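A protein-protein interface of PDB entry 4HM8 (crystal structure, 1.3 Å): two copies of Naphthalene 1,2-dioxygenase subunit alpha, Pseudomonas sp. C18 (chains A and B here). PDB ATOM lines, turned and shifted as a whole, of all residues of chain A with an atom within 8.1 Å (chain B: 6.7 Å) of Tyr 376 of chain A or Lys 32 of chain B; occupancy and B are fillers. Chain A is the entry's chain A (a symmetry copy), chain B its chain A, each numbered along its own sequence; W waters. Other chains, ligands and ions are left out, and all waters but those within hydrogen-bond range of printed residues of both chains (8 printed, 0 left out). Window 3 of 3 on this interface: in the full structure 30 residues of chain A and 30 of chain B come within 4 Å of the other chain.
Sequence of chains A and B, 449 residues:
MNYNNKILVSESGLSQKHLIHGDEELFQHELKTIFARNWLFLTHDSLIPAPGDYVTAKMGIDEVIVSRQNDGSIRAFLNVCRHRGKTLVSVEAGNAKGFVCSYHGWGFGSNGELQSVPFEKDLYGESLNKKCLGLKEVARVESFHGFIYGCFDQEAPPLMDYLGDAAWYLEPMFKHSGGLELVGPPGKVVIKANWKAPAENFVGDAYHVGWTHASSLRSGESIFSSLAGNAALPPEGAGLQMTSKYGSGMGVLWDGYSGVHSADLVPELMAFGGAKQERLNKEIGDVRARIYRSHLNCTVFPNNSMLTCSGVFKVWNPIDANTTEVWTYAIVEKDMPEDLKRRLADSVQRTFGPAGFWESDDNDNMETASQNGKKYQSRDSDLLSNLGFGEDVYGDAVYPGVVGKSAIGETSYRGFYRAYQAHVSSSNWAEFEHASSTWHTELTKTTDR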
ATOM      1  N   GLN A 371     -33.011  11.921 -12.524  1.00  0.00           N
ATOM      2  CA  GLN A 371     -32.973  10.944 -13.597  1.00  0.00           C
ATOM      3  C   GLN A 371     -31.598  10.868 -14.255  1.00  0.00           C
ATOM      4  O   GLN A 371     -31.168   9.799 -14.716  1.00  0.00           O
ATOM      5  CB  GLN A 371     -34.074  11.245 -14.614  1.00  0.00           C
ATOM      6  CG  GLN A 371     -35.474  11.059 -14.023  1.00  0.00           C
ATOM      7  CD  GLN A 371     -36.583  11.612 -14.897  1.00  0.00           C
ATOM      8  OE1 GLN A 371     -36.452  11.673 -16.123  1.00  0.00           O
ATOM      9  NE2 GLN A 371     -37.690  12.009 -14.271  1.00  0.00           N
ATOM     10  N   ASN A 372     -30.889  11.988 -14.281  1.00  0.00           N
ATOM     11  CA  ASN A 372     -29.533  11.980 -14.815  1.00  0.00           C
ATOM     12  C   ASN A 372     -28.590  11.096 -14.002  1.00  0.00           C
ATOM     13  O   ASN A 372     -27.587  10.622 -14.526  1.00  0.00           O
ATOM     14  CB  ASN A 372     -28.982  13.406 -14.942  1.00  0.00           C
ATOM     15  CG  ASN A 372     -29.592  14.157 -16.106  1.00  0.00           C
ATOM     16  OD1 ASN A 372     -30.090  13.552 -17.057  1.00  0.00           O
ATOM     17  ND2 ASN A 372     -29.548  15.475 -16.044  1.00  0.00           N
ATOM     18  N   GLY A 373     -28.920  10.857 -12.733  1.00  0.00           N
ATOM     19  CA  GLY A 373     -28.118   9.983 -11.893  1.00  0.00           C
ATOM     20  C   GLY A 373     -28.133   8.522 -12.315  1.00  0.00           C
ATOM     21  O   GLY A 373     -27.312   7.733 -11.836  1.00  0.00           O
ATOM     22  N   LYS A 374     -29.059   8.154 -13.201  1.00  0.00           N
ATOM     23  CA  LYS A 374     -29.089   6.808 -13.781  1.00  0.00           C
ATOM     24  C   LYS A 374     -28.263   6.712 -15.062  1.00  0.00           C
ATOM     25  O   LYS A 374     -27.892   5.613 -15.484  1.00  0.00           O
ATOM     26  CB  LYS A 374     -30.524   6.391 -14.113  1.00  0.00           C
ATOM     27  CG  LYS A 374     -31.422   6.183 -12.905  1.00  0.00           C
ATOM     28  CD  LYS A 374     -32.773   5.626 -13.322  1.00  0.00           C
ATOM     29  CE  LYS A 374     -33.637   5.235 -12.117  1.00  0.00           C
ATOM     30  NZ  LYS A 374     -33.111   4.012 -11.443  1.00  0.00           N
ATOM     31  N   LYS A 375     -28.000   7.850 -15.703  1.00  0.00           N
ATOM     32  CA  LYS A 375     -27.336   7.841 -17.007  1.00  0.00           C
ATOM     33  C   LYS A 375     -25.873   7.434 -16.878  1.00  0.00           C
ATOM     34  O   LYS A 375     -25.174   7.884 -15.961  1.00  0.00           O
ATOM     35  CB  LYS A 375     -27.473   9.203 -17.691  1.00  0.00           C
ATOM     36  CG  LYS A 375     -28.888   9.505 -18.152  1.00  0.00           C
ATOM     37  CD  LYS A 375     -28.920  10.831 -18.888  1.00  0.00           C
ATOM     38  CE  LYS A 375     -30.151  10.970 -19.753  1.00  0.00           C
ATOM     39  NZ  LYS A 375     -31.377  11.064 -18.932  1.00  0.00           N
ATOM     40  N   TYR A 376     -25.428   6.568 -17.791  1.00  0.00           N
ATOM     41  CA  TYR A 376     -24.130   5.898 -17.667  1.00  0.00           C
ATOM     42  C   TYR A 376     -22.965   6.854 -17.425  1.00  0.00           C
ATOM     43  O   TYR A 376     -22.127   6.614 -16.546  1.00  0.00           O
ATOM     44  CB  TYR A 376     -23.855   5.025 -18.900  1.00  0.00           C
ATOM     45  CG  TYR A 376     -22.551   4.260 -18.804  1.00  0.00           C
ATOM     46  CD1 TYR A 376     -22.486   3.039 -18.150  1.00  0.00           C
ATOM     47  CD2 TYR A 376     -21.377   4.783 -19.329  1.00  0.00           C
ATOM     48  CE1 TYR A 376     -21.285   2.347 -18.043  1.00  0.00           C
ATOM     49  CE2 TYR A 376     -20.179   4.106 -19.224  1.00  0.00           C
ATOM     50  CZ  TYR A 376     -20.133   2.892 -18.579  1.00  0.00           C
ATOM     51  OH  TYR A 376     -18.930   2.221 -18.476  1.00  0.00           O
ATOM     52  N   GLN A 377     -22.882   7.918 -18.221  1.00  0.00           N
ATOM     53  CA  GLN A 377     -21.747   8.845 -18.125  1.00  0.00           C
ATOM     54  C   GLN A 377     -21.827   9.797 -16.937  1.00  0.00           C
ATOM     55  O   GLN A 377     -20.870  10.539 -16.672  1.00  0.00           O
ATOM     56  CB  GLN A 377     -21.590   9.656 -19.425  1.00  0.00           C
ATOM     57  CG  GLN A 377     -21.227   8.823 -20.643  1.00  0.00           C
ATOM     58  CD  GLN A 377     -19.803   8.280 -20.580  1.00  0.00           C
ATOM     59  OE1 GLN A 377     -18.924   8.843 -19.910  1.00  0.00           O
ATOM     60  NE2 GLN A 377     -19.570   7.172 -21.272  1.00  0.00           N
ATOM     61  N   SER A 378     -22.956   9.793 -16.233  1.00  0.00           N
ATOM     62  CA  SER A 378     -23.140  10.679 -15.089  1.00  0.00           C
ATOM     63  C   SER A 378     -23.085   9.988 -13.723  1.00  0.00           C
ATOM     64  O   SER A 378     -22.943  10.666 -12.713  1.00  0.00           O
ATOM     65  CB  SER A 378     -24.447  11.473 -15.207  1.00  0.00           C
ATOM     66  OG  SER A 378     -24.383  12.415 -16.263  1.00  0.00           O
ATOM     67  N   ARG A 379     -23.189   8.660 -13.685  1.00  0.00           N
ATOM     68  CA  ARG A 379     -23.252   7.936 -12.412  1.00  0.00           C
ATOM     69  C   ARG A 379     -22.085   8.271 -11.494  1.00  0.00           C
ATOM     70  O   ARG A 379     -22.284   8.516 -10.300  1.00  0.00           O
ATOM     71  CB  ARG A 379     -23.303   6.428 -12.659  1.00  0.00           C
ATOM     72  CG  ARG A 379     -24.580   5.954 -13.323  1.00  0.00           C
ATOM     73  CD  ARG A 379     -24.468   4.502 -13.782  1.00  0.00           C
ATOM     74  NE  ARG A 379     -25.581   4.142 -14.654  1.00  0.00           N
ATOM     75  CZ  ARG A 379     -25.671   3.002 -15.336  1.00  0.00           C
ATOM     76  NH1 ARG A 379     -24.702   2.089 -15.260  1.00  0.00           N
ATOM     77  NH2 ARG A 379     -26.730   2.782 -16.108  1.00  0.00           N
ATOM     78  N   ASP A 380     -20.882   8.331 -12.071  1.00  0.00           N
ATOM     79  CA  ASP A 380     -19.654   8.552 -11.304  1.00  0.00           C
ATOM     80  C   ASP A 380     -19.240  10.027 -11.296  1.00  0.00           C
ATOM     81  O   ASP A 380     -18.138  10.376 -10.854  1.00  0.00           O
ATOM     82  CB  ASP A 380     -18.530   7.666 -11.875  1.00  0.00           C
ATOM     83  CG  ASP A 380     -17.249   7.722 -11.062  1.00  0.00           C
ATOM     84  OD1 ASP A 380     -17.310   7.597  -9.817  1.00  0.00           O
ATOM     85  OD2 ASP A 380     -16.172   7.898 -11.677  1.00  0.00           O
ATOM     86  N   SER A 381     -20.123  10.903 -11.770  1.00  0.00           N
ATOM     87  CA  SER A 381     -19.825  12.333 -11.748  1.00  0.00           C
ATOM     88  C   SER A 381     -20.094  12.939 -10.373  1.00  0.00           C
ATOM     89  O   SER A 381     -20.783  12.334  -9.535  1.00  0.00           O
ATOM     90  CB  SER A 381     -20.628  13.064 -12.820  1.00  0.00           C
ATOM     91  OG  SER A 381     -20.243  12.606 -14.106  1.00  0.00           O
ATOM     92  N   PHE B  27     -27.772  -5.741 -20.985  1.00  0.00           N
ATOM     93  CA  PHE B  27     -28.016  -4.394 -21.484  1.00  0.00           C
ATOM     94  C   PHE B  27     -27.121  -3.402 -20.735  1.00  0.00           C
ATOM     95  O   PHE B  27     -26.455  -2.560 -21.345  1.00  0.00           O
ATOM     96  CB  PHE B  27     -29.493  -4.009 -21.336  1.00  0.00           C
ATOM     97  CG  PHE B  27     -29.801  -2.615 -21.803  1.00  0.00           C
ATOM     98  CD1 PHE B  27     -29.655  -1.530 -20.941  1.00  0.00           C
ATOM     99  CD2 PHE B  27     -30.225  -2.381 -23.107  1.00  0.00           C
ATOM    100  CE1 PHE B  27     -29.931  -0.229 -21.373  1.00  0.00           C
ATOM    101  CE2 PHE B  27     -30.515  -1.093 -23.544  1.00  0.00           C
ATOM    102  CZ  PHE B  27     -30.371  -0.016 -22.670  1.00  0.00           C
ATOM    103  N   GLN B  28     -27.108  -3.490 -19.411  1.00  0.00           N
ATOM    104  CA  GLN B  28     -26.249  -2.612 -18.619  1.00  0.00           C
ATOM    105  C   GLN B  28     -24.775  -2.786 -19.007  1.00  0.00           C
ATOM    106  O   GLN B  28     -24.026  -1.811 -19.120  1.00  0.00           O
ATOM    107  CB  GLN B  28     -26.475  -2.834 -17.122  1.00  0.00           C
ATOM    108  CG  GLN B  28     -27.869  -2.383 -16.667  1.00  0.00           C
ATOM    109  CD  GLN B  28     -28.058  -0.879 -16.796  1.00  0.00           C
ATOM    110  OE1 GLN B  28     -27.194  -0.099 -16.384  1.00  0.00           O
ATOM    111  NE2 GLN B  28     -29.192  -0.462 -17.365  1.00  0.00           N
ATOM    112  N   HIS B  29     -24.371  -4.024 -19.258  1.00  0.00           N
ATOM    113  CA  HIS B  29     -23.007  -4.302 -19.675  1.00  0.00           C
ATOM    114  C   HIS B  29     -22.713  -3.713 -21.061  1.00  0.00           C
ATOM    115  O   HIS B  29     -21.591  -3.266 -21.317  1.00  0.00           O
ATOM    116  CB  HIS B  29     -22.756  -5.813 -19.646  1.00  0.00           C
ATOM    117  CG  HIS B  29     -21.363  -6.208 -20.018  1.00  0.00           C
ATOM    118  ND1 HIS B  29     -20.277  -5.972 -19.198  1.00  0.00           N
ATOM    119  CD2 HIS B  29     -20.877  -6.845 -21.111  1.00  0.00           C
ATOM    120  CE1 HIS B  29     -19.184  -6.444 -19.774  1.00  0.00           C
ATOM    121  NE2 HIS B  29     -19.520  -6.969 -20.942  1.00  0.00           N
ATOM    122  N   GLU B  30     -23.707  -3.720 -21.949  1.00  0.00           N
ATOM    123  CA  GLU B  30     -23.573  -3.119 -23.274  1.00  0.00           C
ATOM    124  C   GLU B  30     -23.368  -1.615 -23.190  1.00  0.00           C
ATOM    125  O   GLU B  30     -22.711  -1.032 -24.053  1.00  0.00           O
ATOM    126  CB  GLU B  30     -24.805  -3.396 -24.140  1.00  0.00           C
ATOM    127  CG  GLU B  30     -24.981  -4.825 -24.596  1.00  0.00           C
ATOM    128  CD  GLU B  30     -26.292  -5.017 -25.320  1.00  0.00           C
ATOM    129  OE1 GLU B  30     -27.172  -4.134 -25.209  1.00  0.00           O
ATOM    130  OE2 GLU B  30     -26.458  -6.044 -26.010  1.00  0.00           O
ATOM    131  N   LEU B  31     -23.934  -0.973 -22.169  1.00  0.00           N
ATOM    132  CA  LEU B  31     -23.718   0.466 -22.018  1.00  0.00           C
ATOM    133  C   LEU B  31     -22.218   0.753 -21.925  1.00  0.00           C
ATOM    134  O   LEU B  31     -21.718   1.701 -22.539  1.00  0.00           O
ATOM    135  CB  LEU B  31     -24.454   1.025 -20.797  1.00  0.00           C
ATOM    136  CG  LEU B  31     -25.975   0.902 -20.801  1.00  0.00           C
ATOM    137  CD1 LEU B  31     -26.566   1.505 -19.533  1.00  0.00           C
ATOM    138  CD2 LEU B  31     -26.547   1.562 -22.044  1.00  0.00           C
ATOM    139  N   LYS B  32     -21.498  -0.095 -21.191  1.00  0.00           N
ATOM    140  CA  LYS B  32     -20.051   0.042 -21.050  1.00  0.00           C
ATOM    141  C   LYS B  32     -19.266  -0.448 -22.266  1.00  0.00           C
ATOM    142  O   LYS B  32     -18.399   0.267 -22.782  1.00  0.00           O
ATOM    143  CB  LYS B  32     -19.589  -0.700 -19.793  1.00  0.00           C
ATOM    144  CG  LYS B  32     -18.079  -0.746 -19.625  1.00  0.00           C
ATOM    145  CD  LYS B  32     -17.708  -1.324 -18.271  1.00  0.00           C
ATOM    146  CE  LYS B  32     -18.059  -2.795 -18.178  1.00  0.00           C
ATOM    147  NZ  LYS B  32     -17.723  -3.359 -16.834  1.00  0.00           N
ATOM    148  N   THR B  33     -19.570  -1.658 -22.733  1.00  0.00           N
ATOM    149  CA  THR B  33     -18.715  -2.331 -23.726  1.00  0.00           C
ATOM    150  C   THR B  33     -19.113  -2.099 -25.180  1.00  0.00           C
ATOM    151  O   THR B  33     -18.315  -2.339 -26.092  1.00  0.00           O
ATOM    152  CB  THR B  33     -18.622  -3.853 -23.470  1.00  0.00           C
ATOM    153  OG1 THR B  33     -19.928  -4.431 -23.542  1.00  0.00           O
ATOM    154  CG2 THR B  33     -18.001  -4.144 -22.105  1.00  0.00           C
ATOM    155  N   ILE B  34     -20.346  -1.643 -25.397  1.00  0.00           N
ATOM    156  CA  ILE B  34     -20.806  -1.307 -26.742  1.00  0.00           C
ATOM    157  C   ILE B  34     -20.941   0.204 -26.908  1.00  0.00           C
ATOM    158  O   ILE B  34     -20.239   0.806 -27.717  1.00  0.00           O
ATOM    159  CB  ILE B  34     -22.144  -2.003 -27.097  1.00  0.00           C
ATOM    160  CG1 ILE B  34     -21.983  -3.530 -27.044  1.00  0.00           C
ATOM    161  CG2 ILE B  34     -22.640  -1.551 -28.471  1.00  0.00           C
ATOM    162  CD1 ILE B  34     -21.066  -4.107 -28.110  1.00  0.00           C
ATOM    163  N   PHE B  35     -21.820   0.824 -26.127  1.00  0.00           N
ATOM    164  CA  PHE B  35     -22.147   2.230 -26.345  1.00  0.00           C
ATOM    165  C   PHE B  35     -21.109   3.251 -25.877  1.00  0.00           C
ATOM    166  O   PHE B  35     -20.943   4.285 -26.520  1.00  0.00           O
ATOM    167  CB  PHE B  35     -23.555   2.531 -25.814  1.00  0.00           C
ATOM    168  CG  PHE B  35     -24.621   1.763 -26.540  1.00  0.00           C
ATOM    169  CD1 PHE B  35     -25.033   2.159 -27.807  1.00  0.00           C
ATOM    170  CD2 PHE B  35     -25.168   0.608 -25.991  1.00  0.00           C
ATOM    171  CE1 PHE B  35     -26.001   1.438 -28.503  1.00  0.00           C
ATOM    172  CE2 PHE B  35     -26.140  -0.115 -26.672  1.00  0.00           C
ATOM    173  CZ  PHE B  35     -26.544   0.298 -27.940  1.00  0.00           C
ATOM    174  N   ALA B  36     -20.390   2.961 -24.792  1.00  0.00           N
ATOM    175  CA  ALA B  36     -19.346   3.869 -24.318  1.00  0.00           C
ATOM    176  C   ALA B  36     -18.036   3.669 -25.079  1.00  0.00           C
ATOM    177  O   ALA B  36     -17.087   4.443 -24.920  1.00  0.00           O
ATOM    178  CB  ALA B  36     -19.122   3.694 -22.820  1.00  0.00           C
ATOM    179  N   ARG B  37     -17.986   2.632 -25.907  1.00  0.00           N
ATOM    180  CA  ARG B  37     -16.751   2.247 -26.580  1.00  0.00           C
ATOM    181  C   ARG B  37     -16.714   2.551 -28.076  1.00  0.00           C
ATOM    182  O   ARG B  37     -15.646   2.782 -28.654  1.00  0.00           O
ATOM    183  CB  ARG B  37     -16.490   0.758 -26.389  1.00  0.00           C
ATOM    184  CG  ARG B  37     -15.091   0.388 -26.881  1.00  0.00           C
ATOM    185  CD  ARG B  37     -14.725  -1.023 -26.629  1.00  0.00           C
ATOM    186  NE  ARG B  37     -14.755  -1.337 -25.213  1.00  0.00           N
ATOM    187  CZ  ARG B  37     -14.925  -2.564 -24.747  1.00  0.00           C
ATOM    188  NH1 ARG B  37     -15.094  -3.569 -25.601  1.00  0.00           N
ATOM    189  NH2 ARG B  37     -14.947  -2.777 -23.442  1.00  0.00           N
ATOM    190  N   ASN B  38     -17.880   2.519 -28.708  1.00  0.00           N
ATOM    191  CA  ASN B  38     -17.958   2.564 -30.161  1.00  0.00           C
ATOM    192  C   ASN B  38     -18.459   3.903 -30.711  1.00  0.00           C
ATOM    193  O   ASN B  38     -18.867   4.790 -29.945  1.00  0.00           O
ATOM    194  CB  ASN B  38     -18.817   1.400 -30.653  1.00  0.00           C
ATOM    195  CG  ASN B  38     -18.115   0.063 -30.501  1.00  0.00           C
ATOM    196  OD1 ASN B  38     -17.276  -0.284 -31.323  1.00  0.00           O
ATOM    197  ND2 ASN B  38     -18.452  -0.689 -29.448  1.00  0.00           N
ATOM    198  N   MET B  59     -26.490   9.216 -26.997  1.00  0.00           N
ATOM    199  CA  MET B  59     -25.355   8.313 -27.178  1.00  0.00           C
ATOM    200  C   MET B  59     -25.548   7.228 -26.138  1.00  0.00           C
ATOM    201  O   MET B  59     -25.309   7.451 -24.941  1.00  0.00           O
ATOM    202  CB  MET B  59     -24.023   9.039 -26.959  1.00  0.00           C
ATOM    203  CG  MET B  59     -23.647   9.999 -28.080  1.00  0.00           C
ATOM    204  SD  MET B  59     -22.029  10.795 -27.870  1.00  0.00           S
ATOM    205  CE  MET B  59     -20.902   9.400 -27.989  1.00  0.00           C
ATOM    206  N   ILE B  61     -27.696   5.592 -23.534  1.00  0.00           N
ATOM    207  CA  ILE B  61     -28.745   6.226 -22.736  1.00  0.00           C
ATOM    208  C   ILE B  61     -28.404   7.651 -22.310  1.00  0.00           C
ATOM    209  O   ILE B  61     -29.232   8.341 -21.695  1.00  0.00           O
ATOM    210  CB  ILE B  61     -29.142   5.396 -21.495  1.00  0.00           C
ATOM    211  CG1 ILE B  61     -27.984   5.288 -20.492  1.00  0.00           C
ATOM    212  CG2 ILE B  61     -29.633   4.013 -21.917  1.00  0.00           C
ATOM    213  CD1 ILE B  61     -28.404   4.660 -19.170  1.00  0.00           C
ATOM    214  N   ASP B  62     -27.186   8.091 -22.613  1.00  0.00           N
ATOM    215  CA  ASP B  62     -26.779   9.451 -22.288  1.00  0.00           C
ATOM    216  C   ASP B  62     -27.300  10.437 -23.332  1.00  0.00           C
ATOM    217  O   ASP B  62     -27.519  10.069 -24.495  1.00  0.00           O
ATOM    218  CB  ASP B  62     -25.259   9.522 -22.210  1.00  0.00           C
ATOM    219  CG  ASP B  62     -24.713   8.673 -21.091  1.00  0.00           C
ATOM    220  OD1 ASP B  62     -24.778   9.126 -19.931  1.00  0.00           O
ATOM    221  OD2 ASP B  62     -24.228   7.554 -21.360  1.00  0.00           O
ATOM    222  N   LYS B 136     -18.859  17.946 -19.440  1.00  0.00           N
ATOM    223  CA  LYS B 136     -18.129  16.714 -19.726  1.00  0.00           C
ATOM    224  C   LYS B 136     -18.173  16.453 -21.226  1.00  0.00           C
ATOM    225  O   LYS B 136     -19.241  16.240 -21.800  1.00  0.00           O
ATOM    226  CB  LYS B 136     -18.731  15.538 -18.948  1.00  0.00           C
ATOM    227  CG  LYS B 136     -18.062  14.191 -19.213  1.00  0.00           C
ATOM    228  CD  LYS B 136     -18.491  13.154 -18.169  1.00  0.00           C
ATOM    229  CE  LYS B 136     -17.841  11.801 -18.407  1.00  0.00           C
ATOM    230  NZ  LYS B 136     -18.173  10.829 -17.328  1.00  0.00           N
ATOM    231  N   PHE B 152     -17.194   8.123 -26.882  1.00  0.00           N
ATOM    232  CA  PHE B 152     -16.729   8.499 -25.553  1.00  0.00           C
ATOM    233  C   PHE B 152     -15.325   7.969 -25.259  1.00  0.00           C
ATOM    234  O   PHE B 152     -14.678   8.419 -24.315  1.00  0.00           O
ATOM    235  CB  PHE B 152     -17.683   7.970 -24.475  1.00  0.00           C
ATOM    236  CG  PHE B 152     -18.966   8.743 -24.352  1.00  0.00           C
ATOM    237  CD1 PHE B 152     -18.956  10.070 -23.946  1.00  0.00           C
ATOM    238  CD2 PHE B 152     -20.193   8.124 -24.598  1.00  0.00           C
ATOM    239  CE1 PHE B 152     -20.146  10.780 -23.805  1.00  0.00           C
ATOM    240  CE2 PHE B 152     -21.385   8.822 -24.454  1.00  0.00           C
ATOM    241  CZ  PHE B 152     -21.364  10.157 -24.065  1.00  0.00           C
ATOM    242  N   ASP B 153     -14.864   7.014 -26.064  1.00  0.00           N
ATOM    243  CA  ASP B 153     -13.602   6.331 -25.791  1.00  0.00           C
ATOM    244  C   ASP B 153     -12.466   6.921 -26.633  1.00  0.00           C
ATOM    245  O   ASP B 153     -12.414   6.720 -27.850  1.00  0.00           O
ATOM    246  CB  ASP B 153     -13.761   4.834 -26.073  1.00  0.00           C
ATOM    247  CG  ASP B 153     -12.619   3.997 -25.520  1.00  0.00           C
ATOM    248  OD1 ASP B 153     -11.486   4.515 -25.364  1.00  0.00           O
ATOM    249  OD2 ASP B 153     -12.853   2.798 -25.249  1.00  0.00           O
ATOM    250  N   SER B 426     -14.500  -8.042 -23.913  1.00  0.00           N
ATOM    251  CA  SER B 426     -13.259  -7.262 -23.806  1.00  0.00           C
ATOM    252  C   SER B 426     -13.416  -6.046 -22.904  1.00  0.00           C
ATOM    253  O   SER B 426     -14.514  -5.498 -22.791  1.00  0.00           O
ATOM    254  CB  SER B 426     -12.805  -6.800 -25.193  1.00  0.00           C
ATOM    255  OG  SER B 426     -12.418  -7.901 -26.005  1.00  0.00           O
ATOM    256  N   SER B 427     -12.318  -5.617 -22.275  1.00  0.00           N
ATOM    257  CA  SER B 427     -12.357  -4.498 -21.335  1.00  0.00           C
ATOM    258  C   SER B 427     -11.955  -3.175 -21.964  1.00  0.00           C
ATOM    259  O   SER B 427     -12.128  -2.114 -21.361  1.00  0.00           O
ATOM    260  CB  SER B 427     -11.441  -4.775 -20.138  1.00  0.00           C
ATOM    261  OG  SER B 427     -11.862  -5.911 -19.404  1.00  0.00           O
HETATM  262  O   HOH W   1     -25.846  -0.841 -14.070  1.00  0.00           O
HETATM  263  O   HOH W   2     -18.806   9.992 -14.519  1.00  0.00           O
HETATM  264  O   HOH W   3     -23.762  -0.124 -16.844  1.00  0.00           O
HETATM  265  O   HOH W   4     -29.698   2.472 -16.794  1.00  0.00           O
HETATM  266  O   HOH W   5     -25.151  11.622 -18.735  1.00  0.00           O
HETATM  267  O   HOH W   6     -16.958  12.538 -14.970  1.00  0.00           O
HETATM  268  O   HOH W   7     -31.526   7.928 -20.432  1.00  0.00           O
HETATM  269  O   HOH W   8     -17.018   8.122 -17.248  1.00  0.00           O
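The side-chain amide oxygen of Gln 28 of chain B lies within hydrogen-bond range of the guanidinium group of Arg 379 of chain A (2.9 Å). The backbone NH (N) of Tyr 376 of chain A sits at hydrogen-bond distance from the side-chain carboxylate (OD1) of Asp 62 of chain B (3.4 Å). The backbone NH (N) of Gln 377 of chain A lies within hydrogen-bond range of the side-chain carboxylate (OD1) of Asp 62 of chain B (2.8 Å). NZ of Lys 136 of chain B is in hydrogen-bond range of O of Gln 377 of chain A (2.8 Å).
The backbone carbonyl oxygen (O) of Leu 31 of chain B sits at hydrogen-bond distance from the backbone NH (N) of Ala 36 of chain B (2.9 Å). OD1 of Asn 372 of chain A lies within hydrogen-bond range of NZ of Lys 375 of chain A, 3.4 Å away. The guanidinium group (NE) of Arg 379 of chain A sits at hydrogen-bond distance from the backbone carbonyl oxygen (O) of Lys 374 of chain A (2.9 Å). The backbone carbonyl oxygen (O) of Gln 377 of chain A is in hydrogen-bond range of the side-chain hydroxyl (OG) of Ser 381 of chain A, 3.4 Å away.
Lys 374 of chain A touches Ile 61 of chain B. CE of Lys 375 of chain A touches O of Ile 61 of chain B (3.4 Å). Asp 62 of chain B touches Lys 375 of chain A (OD1 to CB, 3.5 Å). Leu 31 of chain B touches Tyr 376 of chain A. OH of Tyr 376 of chain A touches CB of Lys 32 of chain B, at 3.3 Å. Tyr 376 of chain A touches Ala 36 of chain B (CE2 to CB, 3.8 Å). Gln 377 of chain A touches Ala 36 of chain B. NE2 of Gln 377 of chain A touches CG of Phe 152 of chain B, 3.5 Å away. Leu 31 of chain B touches Arg 379 of chain A (CD1 to NH2, 3.7 Å). NH2 of Arg 379 of chain A touches CD1 of Ile 61 of chain B, 3.96 Å away.
Of chain B, only Leu 31, Lys 32, Ala 36, Ile 61 and Asp 62 come within 4 Å of Tyr 376 of chain A. Of chain A, only Tyr 376 comes within 4 Å of Lys 32 of chain B. Of the printed residues of chain A, Ala 36 of chain B touches Tyr 376 (3.8 Å) and Gln 377 (3.8 Å). Printed residues of chain B within 4 Å of Arg 379 of chain A: Gln 28, Leu 31 and Ile 61. Asn 38 of chain B touches none of the printed residues of chain A. Ile 34 of chain B touches none of the printed residues of chain A. The nearest residue of chain B that does not touch Tyr 376 of chain A is Gln 28 of chain B (5.1 Å). The nearest residue of chain A that does not touch Lys 32 of chain B is Arg 379 of chain A (7.1 Å). The nearest printed residue of chain B that does not touch Lys 375 of chain A is Leu 31 of chain B (6.5 Å).
Of the 20 printed residues of chain B, 8 touch a printed residue of chain A. Hydrophobic or aromatic side chains of chain B within 4 Å of the printed part of chain A: Leu 31, Ala 36, Ile 61 and Phe 152. Along chain B the printed residues that touch a printed residue of chain A span positions 28 to 152. Hydrophobic or aromatic side chains of chain A within 4 Å of the printed part of chain B: Tyr 376.
No position is printed for both chains. Of the 15 pairs that touch across the chains among the printed residues, none has its exchanged pair printed and touching as well.
Water W7 lies within hydrogen-bond range of the backbone carbonyl oxygen (O) of Ile 61 of chain B and the side-chain amino group (NZ) of Lys 375 of chain A. Water W5 bridges OG of Ser 378 of chain A and OD1 of Asp 62 of chain B. Water W1 bridges the side-chain amide oxygen (OE1) of Gln 28 of chain B (2.8 Å) and the guanidinium group (NH1) of Arg 379 of chain A (3.4 Å). Water W8 bridges the side-chain amino group of Lys 136 of chain B (2.9 Å) and the side-chain amide oxygen of Gln 377 of chain A (3.4 Å). Water W2 lies within hydrogen-bond range of NZ of Lys 136 of chain B (3.0 Å), OG of Ser 381 of chain A (3.0 Å) and O of Gln 377 of chain A (3.0 Å). Water W6 lies within hydrogen-bond range of NZ of Lys 136 of chain B (3.2 Å) and OG of Ser 381 of chain A (3.4 Å).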
